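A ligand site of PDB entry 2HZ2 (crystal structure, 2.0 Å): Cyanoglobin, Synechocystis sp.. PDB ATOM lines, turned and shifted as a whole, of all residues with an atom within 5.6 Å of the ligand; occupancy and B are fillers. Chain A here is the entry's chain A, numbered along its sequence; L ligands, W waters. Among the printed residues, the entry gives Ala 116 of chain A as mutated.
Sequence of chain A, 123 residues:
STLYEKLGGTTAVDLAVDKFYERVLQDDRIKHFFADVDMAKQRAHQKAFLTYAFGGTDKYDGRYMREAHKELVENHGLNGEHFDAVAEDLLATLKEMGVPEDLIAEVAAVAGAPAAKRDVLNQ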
ATOM      1  N   ILE A  30      37.451   5.347  -2.608  1.00  0.00           N
ATOM      2  CA  ILE A  30      36.361   4.842  -3.472  1.00  0.00           C
ATOM      3  C   ILE A  30      36.173   5.587  -4.787  1.00  0.00           C
ATOM      4  O   ILE A  30      35.446   5.160  -5.672  1.00  0.00           O
ATOM      5  CB  ILE A  30      35.071   4.754  -2.679  1.00  0.00           C
ATOM      6  CG1 ILE A  30      34.770   6.069  -1.981  1.00  0.00           C
ATOM      7  CG2 ILE A  30      35.185   3.678  -1.615  1.00  0.00           C
ATOM      8  CD1 ILE A  30      33.360   6.084  -1.334  1.00  0.00           C
ATOM      9  N   PHE A  33      36.171   3.684  -8.305  1.00  0.00           N
ATOM     10  CA  PHE A  33      35.051   2.857  -8.753  1.00  0.00           C
ATOM     11  C   PHE A  33      34.192   3.610  -9.779  1.00  0.00           C
ATOM     12  O   PHE A  33      33.510   2.964 -10.514  1.00  0.00           O
ATOM     13  CB  PHE A  33      34.217   2.397  -7.568  1.00  0.00           C
ATOM     14  CG  PHE A  33      34.967   1.441  -6.650  1.00  0.00           C
ATOM     15  CD1 PHE A  33      35.196   0.129  -7.024  1.00  0.00           C
ATOM     16  CD2 PHE A  33      35.535   1.897  -5.480  1.00  0.00           C
ATOM     17  CE1 PHE A  33      35.907  -0.717  -6.231  1.00  0.00           C
ATOM     18  CE2 PHE A  33      36.276   1.057  -4.715  1.00  0.00           C
ATOM     19  CZ  PHE A  33      36.441  -0.263  -5.085  1.00  0.00           C
ATOM     20  N   PHE A  34      34.232   4.950  -9.785  1.00  0.00           N
ATOM     21  CA  PHE A  34      33.436   5.819 -10.667  1.00  0.00           C
ATOM     22  C   PHE A  34      34.238   6.319 -11.897  1.00  0.00           C
ATOM     23  O   PHE A  34      33.787   7.236 -12.631  1.00  0.00           O
ATOM     24  CB  PHE A  34      32.860   6.994  -9.847  1.00  0.00           C
ATOM     25  CG  PHE A  34      31.994   6.560  -8.739  1.00  0.00           C
ATOM     26  CD1 PHE A  34      32.509   6.386  -7.488  1.00  0.00           C
ATOM     27  CD2 PHE A  34      30.680   6.251  -8.958  1.00  0.00           C
ATOM     28  CE1 PHE A  34      31.699   5.898  -6.440  1.00  0.00           C
ATOM     29  CE2 PHE A  34      29.871   5.738  -7.932  1.00  0.00           C
ATOM     30  CZ  PHE A  34      30.379   5.591  -6.675  1.00  0.00           C
ATOM     31  N   VAL A  37      32.364   6.175 -15.070  1.00  0.00           N
ATOM     32  CA  VAL A  37      30.993   6.623 -14.826  1.00  0.00           C
ATOM     33  C   VAL A  37      30.918   8.161 -15.027  1.00  0.00           C
ATOM     34  O   VAL A  37      31.617   8.936 -14.409  1.00  0.00           O
ATOM     35  CB  VAL A  37      30.516   6.199 -13.399  1.00  0.00           C
ATOM     36  CG1 VAL A  37      29.077   6.586 -13.151  1.00  0.00           C
ATOM     37  CG2 VAL A  37      30.723   4.707 -13.189  1.00  0.00           C
ATOM     38  N   LYS A  41      25.583  10.012 -13.857  1.00  0.00           N
ATOM     39  CA  LYS A  41      25.439   8.729 -13.190  1.00  0.00           C
ATOM     40  C   LYS A  41      26.076   8.773 -11.790  1.00  0.00           C
ATOM     41  O   LYS A  41      25.566   8.165 -10.876  1.00  0.00           O
ATOM     42  CB  LYS A  41      26.043   7.559 -14.002  1.00  0.00           C
ATOM     43  CG  LYS A  41      25.171   6.926 -15.138  1.00  0.00           C
ATOM     44  CD  LYS A  41      23.684   6.793 -14.826  1.00  0.00           C
ATOM     45  CE  LYS A  41      23.312   5.550 -13.995  1.00  0.00           C
ATOM     46  NZ  LYS A  41      22.160   5.861 -13.044  1.00  0.00           N
ATOM     47  N   GLN A  42      27.181   9.504 -11.612  1.00  0.00           N
ATOM     48  CA  GLN A  42      27.863   9.530 -10.342  1.00  0.00           C
ATOM     49  C   GLN A  42      26.952  10.170  -9.306  1.00  0.00           C
ATOM     50  O   GLN A  42      26.727   9.651  -8.166  1.00  0.00           O
ATOM     51  CB  GLN A  42      29.165  10.274 -10.458  1.00  0.00           C
ATOM     52  CG  GLN A  42      30.219   9.490 -11.246  1.00  0.00           C
ATOM     53  CD  GLN A  42      31.473  10.308 -11.469  1.00  0.00           C
ATOM     54  OE1 GLN A  42      31.546  11.453 -11.001  1.00  0.00           O
ATOM     55  NE2 GLN A  42      32.460   9.719 -12.172  1.00  0.00           N
ATOM     56  N   HIS A  45      24.011   8.054  -8.432  1.00  0.00           N
ATOM     57  CA  HIS A  45      24.342   6.923  -7.611  1.00  0.00           C
ATOM     58  C   HIS A  45      24.277   7.296  -6.135  1.00  0.00           C
ATOM     59  O   HIS A  45      23.805   6.537  -5.307  1.00  0.00           O
ATOM     60  CB  HIS A  45      25.753   6.386  -7.915  1.00  0.00           C
ATOM     61  CG  HIS A  45      26.073   5.199  -7.086  1.00  0.00           C
ATOM     62  ND1 HIS A  45      26.593   5.281  -5.805  1.00  0.00           N
ATOM     63  CD2 HIS A  45      25.778   3.892  -7.286  1.00  0.00           C
ATOM     64  CE1 HIS A  45      26.682   4.071  -5.305  1.00  0.00           C
ATOM     65  NE2 HIS A  45      26.185   3.208  -6.165  1.00  0.00           N
ATOM     66  N   ALA A  48      20.761   7.597  -5.148  1.00  0.00           N
ATOM     67  CA  ALA A  48      20.308   6.253  -4.880  1.00  0.00           C
ATOM     68  C   ALA A  48      20.683   5.666  -3.510  1.00  0.00           C
ATOM     69  O   ALA A  48      19.826   5.153  -2.815  1.00  0.00           O
ATOM     70  CB  ALA A  48      20.822   5.362  -5.952  1.00  0.00           C
ATOM     71  N   PHE A  49      21.964   5.665  -3.183  1.00  0.00           N
ATOM     72  CA  PHE A  49      22.444   5.174  -1.918  1.00  0.00           C
ATOM     73  C   PHE A  49      21.740   5.924  -0.729  1.00  0.00           C
ATOM     74  O   PHE A  49      21.385   5.313   0.321  1.00  0.00           O
ATOM     75  CB  PHE A  49      23.940   5.329  -1.813  1.00  0.00           C
ATOM     76  CG  PHE A  49      24.518   4.683  -0.582  1.00  0.00           C
ATOM     77  CD1 PHE A  49      24.912   3.337  -0.580  1.00  0.00           C
ATOM     78  CD2 PHE A  49      24.688   5.399   0.568  1.00  0.00           C
ATOM     79  CE1 PHE A  49      25.447   2.730   0.599  1.00  0.00           C
ATOM     80  CE2 PHE A  49      25.222   4.827   1.722  1.00  0.00           C
ATOM     81  CZ  PHE A  49      25.602   3.488   1.742  1.00  0.00           C
ATOM     82  N   TYR A  52      18.185   4.690  -0.485  1.00  0.00           N
ATOM     83  CA  TYR A  52      18.283   3.415   0.175  1.00  0.00           C
ATOM     84  C   TYR A  52      18.421   3.519   1.699  1.00  0.00           C
ATOM     85  O   TYR A  52      17.620   2.937   2.456  1.00  0.00           O
ATOM     86  CB  TYR A  52      19.415   2.597  -0.453  1.00  0.00           C
ATOM     87  CG  TYR A  52      19.778   1.408   0.365  1.00  0.00           C
ATOM     88  CD1 TYR A  52      18.992   0.268   0.376  1.00  0.00           C
ATOM     89  CD2 TYR A  52      20.898   1.433   1.171  1.00  0.00           C
ATOM     90  CE1 TYR A  52      19.329  -0.782   1.182  1.00  0.00           C
ATOM     91  CE2 TYR A  52      21.237   0.384   1.939  1.00  0.00           C
ATOM     92  CZ  TYR A  52      20.469  -0.729   1.922  1.00  0.00           C
ATOM     93  OH  TYR A  52      20.832  -1.742   2.749  1.00  0.00           O
ATOM     94  N   TYR A  60      15.708  -1.335  -4.742  1.00  0.00           N
ATOM     95  CA  TYR A  60      17.060  -1.876  -4.739  1.00  0.00           C
ATOM     96  C   TYR A  60      16.998  -3.367  -4.307  1.00  0.00           C
ATOM     97  O   TYR A  60      17.566  -3.784  -3.298  1.00  0.00           O
ATOM     98  CB  TYR A  60      18.006  -0.971  -3.918  1.00  0.00           C
ATOM     99  CG  TYR A  60      17.868   0.533  -4.294  1.00  0.00           C
ATOM    100  CD1 TYR A  60      17.326   1.451  -3.425  1.00  0.00           C
ATOM    101  CD2 TYR A  60      18.209   0.981  -5.550  1.00  0.00           C
ATOM    102  CE1 TYR A  60      17.159   2.792  -3.772  1.00  0.00           C
ATOM    103  CE2 TYR A  60      18.042   2.327  -5.920  1.00  0.00           C
ATOM    104  CZ  TYR A  60      17.528   3.223  -5.027  1.00  0.00           C
ATOM    105  OH  TYR A  60      17.327   4.512  -5.406  1.00  0.00           O
ATOM    106  N   TYR A  64      19.243  -7.096  -8.268  1.00  0.00           N
ATOM    107  CA  TYR A  64      19.669  -5.964  -9.054  1.00  0.00           C
ATOM    108  C   TYR A  64      21.000  -5.428  -8.485  1.00  0.00           C
ATOM    109  O   TYR A  64      21.941  -5.092  -9.231  1.00  0.00           O
ATOM    110  CB  TYR A  64      18.554  -4.916  -9.030  1.00  0.00           C
ATOM    111  CG  TYR A  64      18.843  -3.577  -9.661  1.00  0.00           C
ATOM    112  CD1 TYR A  64      19.680  -3.454 -10.749  1.00  0.00           C
ATOM    113  CD2 TYR A  64      18.201  -2.438  -9.200  1.00  0.00           C
ATOM    114  CE1 TYR A  64      19.913  -2.211 -11.343  1.00  0.00           C
ATOM    115  CE2 TYR A  64      18.423  -1.208  -9.754  1.00  0.00           C
ATOM    116  CZ  TYR A  64      19.287  -1.100 -10.842  1.00  0.00           C
ATOM    117  OH  TYR A  64      19.505   0.129 -11.426  1.00  0.00           O
ATOM    118  N   MET A  65      21.092  -5.398  -7.167  1.00  0.00           N
ATOM    119  CA  MET A  65      22.312  -4.915  -6.491  1.00  0.00           C
ATOM    120  C   MET A  65      23.478  -5.819  -6.847  1.00  0.00           C
ATOM    121  O   MET A  65      24.553  -5.350  -7.107  1.00  0.00           O
ATOM    122  CB  MET A  65      22.128  -4.825  -4.983  1.00  0.00           C
ATOM    123  CG  MET A  65      21.254  -3.663  -4.508  1.00  0.00           C
ATOM    124  SD  MET A  65      21.638  -2.014  -5.152  1.00  0.00           S
ATOM    125  CE  MET A  65      20.825  -2.067  -6.695  1.00  0.00           C
ATOM    126  N   ALA A  68      24.384  -5.235 -10.554  1.00  0.00           N
ATOM    127  CA  ALA A  68      24.849  -3.838 -10.843  1.00  0.00           C
ATOM    128  C   ALA A  68      26.307  -3.646 -10.428  1.00  0.00           C
ATOM    129  O   ALA A  68      27.009  -2.819 -11.001  1.00  0.00           O
ATOM    130  CB  ALA A  68      23.951  -2.766 -10.138  1.00  0.00           C
ATOM    131  N   HIS A  69      26.756  -4.376  -9.385  1.00  0.00           N
ATOM    132  CA  HIS A  69      28.112  -4.222  -8.852  1.00  0.00           C
ATOM    133  C   HIS A  69      29.074  -5.325  -9.201  1.00  0.00           C
ATOM    134  O   HIS A  69      30.214  -5.299  -8.756  1.00  0.00           O
ATOM    135  CB  HIS A  69      28.071  -4.060  -7.342  1.00  0.00           C
ATOM    136  CG  HIS A  69      27.198  -2.941  -6.936  1.00  0.00           C
ATOM    137  ND1 HIS A  69      25.842  -3.069  -6.826  1.00  0.00           N
ATOM    138  CD2 HIS A  69      27.475  -1.627  -6.784  1.00  0.00           C
ATOM    139  CE1 HIS A  69      25.325  -1.889  -6.504  1.00  0.00           C
ATOM    140  NE2 HIS A  69      26.301  -1.009  -6.486  1.00  0.00           N
ATOM    141  N   LEU A  72      32.441  -4.300 -10.580  1.00  0.00           N
ATOM    142  CA  LEU A  72      33.240  -3.667  -9.548  1.00  0.00           C
ATOM    143  C   LEU A  72      33.921  -4.704  -8.673  1.00  0.00           C
ATOM    144  O   LEU A  72      35.124  -4.600  -8.333  1.00  0.00           O
ATOM    145  CB  LEU A  72      32.350  -2.802  -8.715  1.00  0.00           C
ATOM    146  CG  LEU A  72      31.613  -1.674  -9.437  1.00  0.00           C
ATOM    147  CD1 LEU A  72      30.956  -0.815  -8.312  1.00  0.00           C
ATOM    148  CD2 LEU A  72      32.479  -0.810 -10.344  1.00  0.00           C
ATOM    149  N   LEU A  78      36.223  -4.403  -5.508  1.00  0.00           N
ATOM    150  CA  LEU A  78      35.266  -3.887  -4.530  1.00  0.00           C
ATOM    151  C   LEU A  78      35.098  -4.870  -3.331  1.00  0.00           C
ATOM    152  O   LEU A  78      34.824  -6.065  -3.509  1.00  0.00           O
ATOM    153  CB  LEU A  78      33.907  -3.650  -5.177  1.00  0.00           C
ATOM    154  CG  LEU A  78      32.798  -3.076  -4.283  1.00  0.00           C
ATOM    155  CD1 LEU A  78      33.141  -1.667  -3.930  1.00  0.00           C
ATOM    156  CD2 LEU A  78      31.343  -3.169  -4.926  1.00  0.00           C
ATOM    157  N   HIS A  82      35.438  -0.735   1.131  1.00  0.00           N
ATOM    158  CA  HIS A  82      34.822   0.256   0.232  1.00  0.00           C
ATOM    159  C   HIS A  82      33.381   0.506   0.579  1.00  0.00           C
ATOM    160  O   HIS A  82      32.963   1.661   0.637  1.00  0.00           O
ATOM    161  CB  HIS A  82      34.961  -0.184  -1.231  1.00  0.00           C
ATOM    162  CG  HIS A  82      36.352  -0.527  -1.586  1.00  0.00           C
ATOM    163  ND1 HIS A  82      36.790  -1.818  -1.802  1.00  0.00           N
ATOM    164  CD2 HIS A  82      37.441   0.270  -1.702  1.00  0.00           C
ATOM    165  CE1 HIS A  82      38.074  -1.795  -2.044  1.00  0.00           C
ATOM    166  NE2 HIS A  82      38.502  -0.556  -1.959  1.00  0.00           N
ATOM    167  N   PHE A  83      32.617  -0.562   0.815  1.00  0.00           N
ATOM    168  CA  PHE A  83      31.203  -0.449   1.137  1.00  0.00           C
ATOM    169  C   PHE A  83      31.016   0.434   2.386  1.00  0.00           C
ATOM    170  O   PHE A  83      30.201   1.367   2.408  1.00  0.00           O
ATOM    171  CB  PHE A  83      30.605  -1.823   1.354  1.00  0.00           C
ATOM    172  CG  PHE A  83      29.126  -1.834   1.476  1.00  0.00           C
ATOM    173  CD1 PHE A  83      28.513  -1.431   2.679  1.00  0.00           C
ATOM    174  CD2 PHE A  83      28.334  -2.179   0.398  1.00  0.00           C
ATOM    175  CE1 PHE A  83      27.096  -1.425   2.788  1.00  0.00           C
ATOM    176  CE2 PHE A  83      26.925  -2.182   0.496  1.00  0.00           C
ATOM    177  CZ  PHE A  83      26.300  -1.801   1.681  1.00  0.00           C
ATOM    178  N   VAL A  86      31.543   4.237   1.896  1.00  0.00           N
ATOM    179  CA  VAL A  86      30.437   4.984   1.312  1.00  0.00           C
ATOM    180  C   VAL A  86      29.449   5.357   2.418  1.00  0.00           C
ATOM    181  O   VAL A  86      28.982   6.494   2.498  1.00  0.00           O
ATOM    182  CB  VAL A  86      29.665   4.200   0.186  1.00  0.00           C
ATOM    183  CG1 VAL A  86      28.409   4.964  -0.278  1.00  0.00           C
ATOM    184  CG2 VAL A  86      30.565   3.927  -1.084  1.00  0.00           C
ATOM    185  N   ALA A 111      22.050   1.728   6.089  1.00  0.00           N
ATOM    186  CA  ALA A 111      23.229   1.775   5.200  1.00  0.00           C
ATOM    187  C   ALA A 111      24.095   0.538   5.375  1.00  0.00           C
ATOM    188  O   ALA A 111      24.545  -0.039   4.398  1.00  0.00           O
ATOM    189  CB  ALA A 111      24.051   2.977   5.434  1.00  0.00           C
ATOM    190  N   ALA A 116      21.847  -6.629   2.198  1.00  0.00           N
ATOM    191  CA  ALA A 116      22.116  -5.801   0.995  1.00  0.00           C
ATOM    192  C   ALA A 116      23.606  -5.683   0.717  1.00  0.00           C
ATOM    193  O   ALA A 116      24.033  -5.699  -0.447  1.00  0.00           O
ATOM    194  CB  ALA A 116      21.509  -4.405   1.134  1.00  0.00           C
ATOM    195  N   LYS A 117      24.402  -5.609   1.778  1.00  0.00           N
ATOM    196  CA  LYS A 117      25.872  -5.563   1.689  1.00  0.00           C
ATOM    197  C   LYS A 117      26.420  -6.822   1.009  1.00  0.00           C
ATOM    198  O   LYS A 117      27.212  -6.757   0.059  1.00  0.00           O
ATOM    199  CB  LYS A 117      26.472  -5.392   3.116  1.00  0.00           C
ATOM    200  CG  LYS A 117      27.988  -5.310   3.140  1.00  0.00           C
ATOM    201  CD  LYS A 117      28.542  -4.770   4.477  1.00  0.00           C
ATOM    202  CE  LYS A 117      30.028  -4.664   4.373  1.00  0.00           C
ATOM    203  NZ  LYS A 117      30.768  -4.398   5.601  1.00  0.00           N
ATOM    204  N   VAL A 120      25.491  -6.476  -2.895  1.00  0.00           N
ATOM    205  CA  VAL A 120      26.390  -5.510  -3.569  1.00  0.00           C
ATOM    206  C   VAL A 120      27.799  -6.138  -3.743  1.00  0.00           C
ATOM    207  O   VAL A 120      28.412  -6.072  -4.844  1.00  0.00           O
ATOM    208  CB  VAL A 120      26.475  -4.167  -2.728  1.00  0.00           C
ATOM    209  CG1 VAL A 120      27.629  -3.282  -3.240  1.00  0.00           C
ATOM    210  CG2 VAL A 120      25.161  -3.400  -2.792  1.00  0.00           C
HETATM  211  C1  LIG L   1      25.562   1.248  -9.695  1.00  0.00           C
HETATM  212  C2  LIG L   1      22.866   1.132  -5.749  1.00  0.00           C
HETATM  213  C3  LIG L   1      26.811   0.434  -3.092  1.00  0.00           C
HETATM  214  C4  LIG L   1      29.426   1.889  -6.820  1.00  0.00           C
HETATM  215  C5  LIG L   1      24.524   1.211  -8.832  1.00  0.00           C
HETATM  216  C6  LIG L   1      23.160   1.176  -9.245  1.00  0.00           C
HETATM  217  C7  LIG L   1      22.409   1.295  -8.153  1.00  0.00           C
HETATM  218  C8  LIG L   1      23.305   1.288  -7.028  1.00  0.00           C
HETATM  219  C9  LIG L   1      20.879   1.460  -8.228  1.00  0.00           C
HETATM  220  C10 LIG L   1      22.652   0.911 -10.657  1.00  0.00           C
HETATM  221  C11 LIG L   1      22.524   2.047 -11.577  1.00  0.00           C
HETATM  222  C12 LIG L   1      22.143   1.546 -12.996  1.00  0.00           C
HETATM  223  O1  LIG L   1      21.532   0.452 -13.216  1.00  0.00           O
HETATM  224  O2  LIG L   1      22.512   2.303 -13.923  1.00  0.00           O
HETATM  225  C13 LIG L   1      23.709   0.952  -4.669  1.00  0.00           C
HETATM  226  C14 LIG L   1      23.246   0.716  -3.362  1.00  0.00           C
HETATM  227  C15 LIG L   1      24.359   0.522  -2.612  1.00  0.00           C
HETATM  228  C16 LIG L   1      25.499   0.563  -3.519  1.00  0.00           C
HETATM  229  C17 LIG L   1      21.786   0.719  -2.872  1.00  0.00           C
HETATM  230  C18 LIG L   1      24.480   0.065  -1.291  1.00  0.00           C
HETATM  231  C19 LIG L   1      23.434  -0.693  -0.663  1.00  0.00           C
HETATM  232  C20 LIG L   1      27.912   0.775  -3.852  1.00  0.00           C
HETATM  233  C21 LIG L   1      29.288   0.850  -3.375  1.00  0.00           C
HETATM  234  C22 LIG L   1      29.997   1.367  -4.457  1.00  0.00           C
HETATM  235  C23 LIG L   1      29.066   1.522  -5.546  1.00  0.00           C
HETATM  236  C24 LIG L   1      29.728   0.410  -1.988  1.00  0.00           C
HETATM  237  C25 LIG L   1      31.328   1.798  -4.642  1.00  0.00           C
HETATM  238  C26 LIG L   1      32.309   1.926  -3.622  1.00  0.00           C
HETATM  239  C27 LIG L   1      28.595   1.813  -7.906  1.00  0.00           C
HETATM  240  C28 LIG L   1      29.039   1.837  -9.287  1.00  0.00           C
HETATM  241  C29 LIG L   1      27.982   1.617 -10.089  1.00  0.00           C
HETATM  242  C30 LIG L   1      26.878   1.434  -9.242  1.00  0.00           C
HETATM  243  C31 LIG L   1      30.433   2.250  -9.771  1.00  0.00           C
HETATM  244  C32 LIG L   1      27.989   1.681 -11.609  1.00  0.00           C
HETATM  245  C33 LIG L   1      28.037   3.108 -12.039  1.00  0.00           C
HETATM  246  C34 LIG L   1      26.817   3.861 -11.667  1.00  0.00           C
HETATM  247  O3  LIG L   1      26.935   4.859 -10.878  1.00  0.00           O
HETATM  248  O4  LIG L   1      25.749   3.465 -12.212  1.00  0.00           O
HETATM  249  N1  LIG L   1      24.595   1.269  -7.465  1.00  0.00           N
HETATM  250  N2  LIG L   1      25.097   0.894  -4.781  1.00  0.00           N
HETATM  251  N3  LIG L   1      27.811   1.171  -5.184  1.00  0.00           N
HETATM  252  N4  LIG L   1      27.266   1.534  -7.891  1.00  0.00           N
HETATM  253 FE1  LIG L   1      26.209   1.158  -6.339  1.00  0.00          FE
HETATM  254  O   HOH W   1      26.701   3.027 -14.493  1.00  0.00           O
HETATM  255  O   HOH W   2      22.800   4.585  -8.975  1.00  0.00           O
HETATM  256  O   HOH W   3      24.209   5.608 -11.099  1.00  0.00           O
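Merely in contact with the ligand: Phe 33 (3.2 Å), Val 37 (3.3 Å), Phe 49 (3.4 Å), Leu 72 (3.4 Å), Met 65 (3.4 Å), Phe 83 (3.6 Å), Tyr 52 (3.6 Å), Val 86 (3.7 Å), Leu 78 (3.7 Å), Tyr 60 (3.8 Å), Val 120 (3.8 Å), Phe 34 (3.8 Å), Ile 30 (3.9 Å) and Ala 68 (3.9 Å). Hydrophobic or aromatic side chains that line the ligand: Ile 30, Phe 33, Phe 34, Val 37, His 45, Phe 49, Tyr 52, Tyr 60, Tyr 64, Met 65, Ala 68, His 69, Leu 72, Leu 78, Phe 83, Val 86 and Val 120. Within 4 Å of the ligand: Ile 30, Phe 33, Phe 34, Val 37, Lys 41, His 45, Phe 49, Tyr 52, Tyr 60, Tyr 64, Met 65, Ala 68, His 69, Leu 72, Leu 78, Phe 83, Val 86 and Val 120. The nearest printed residue that does not touch the ligand is His 82 (4.1 Å).
Water W3 lies within hydrogen-bond range of an oxygen (O3) of the ligand and the side-chain amino group (NZ) of Lys 41.
O of Leu 72 sits at hydrogen-bond distance from N of Leu 78 (3.0 Å). ND1 of His 69 lies within hydrogen-bond range of O of Met 65, at 2.6 Å. The backbone carbonyl oxygen (O) of Phe 34 sits at hydrogen-bond distance from the side-chain amide nitrogen (NE2) of Gln 42 (2.9 Å). The backbone carbonyl oxygen of Val 37 lies within hydrogen-bond range of the side-chain amide nitrogen of Gln 42 (2.5 Å).
O1 of the ligand sits at hydrogen-bond distance from OH of Tyr 64, at 2.7 Å. O2 of the ligand lies within salt-bridge range of NZ of Lys 41, 3.7 Å away. NE2 of His 45 is bound to FE1 of the ligand. A ring nitrogen (NE2) of His 69 binds an iron atom (FE1) of the ligand (2.2 Å).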
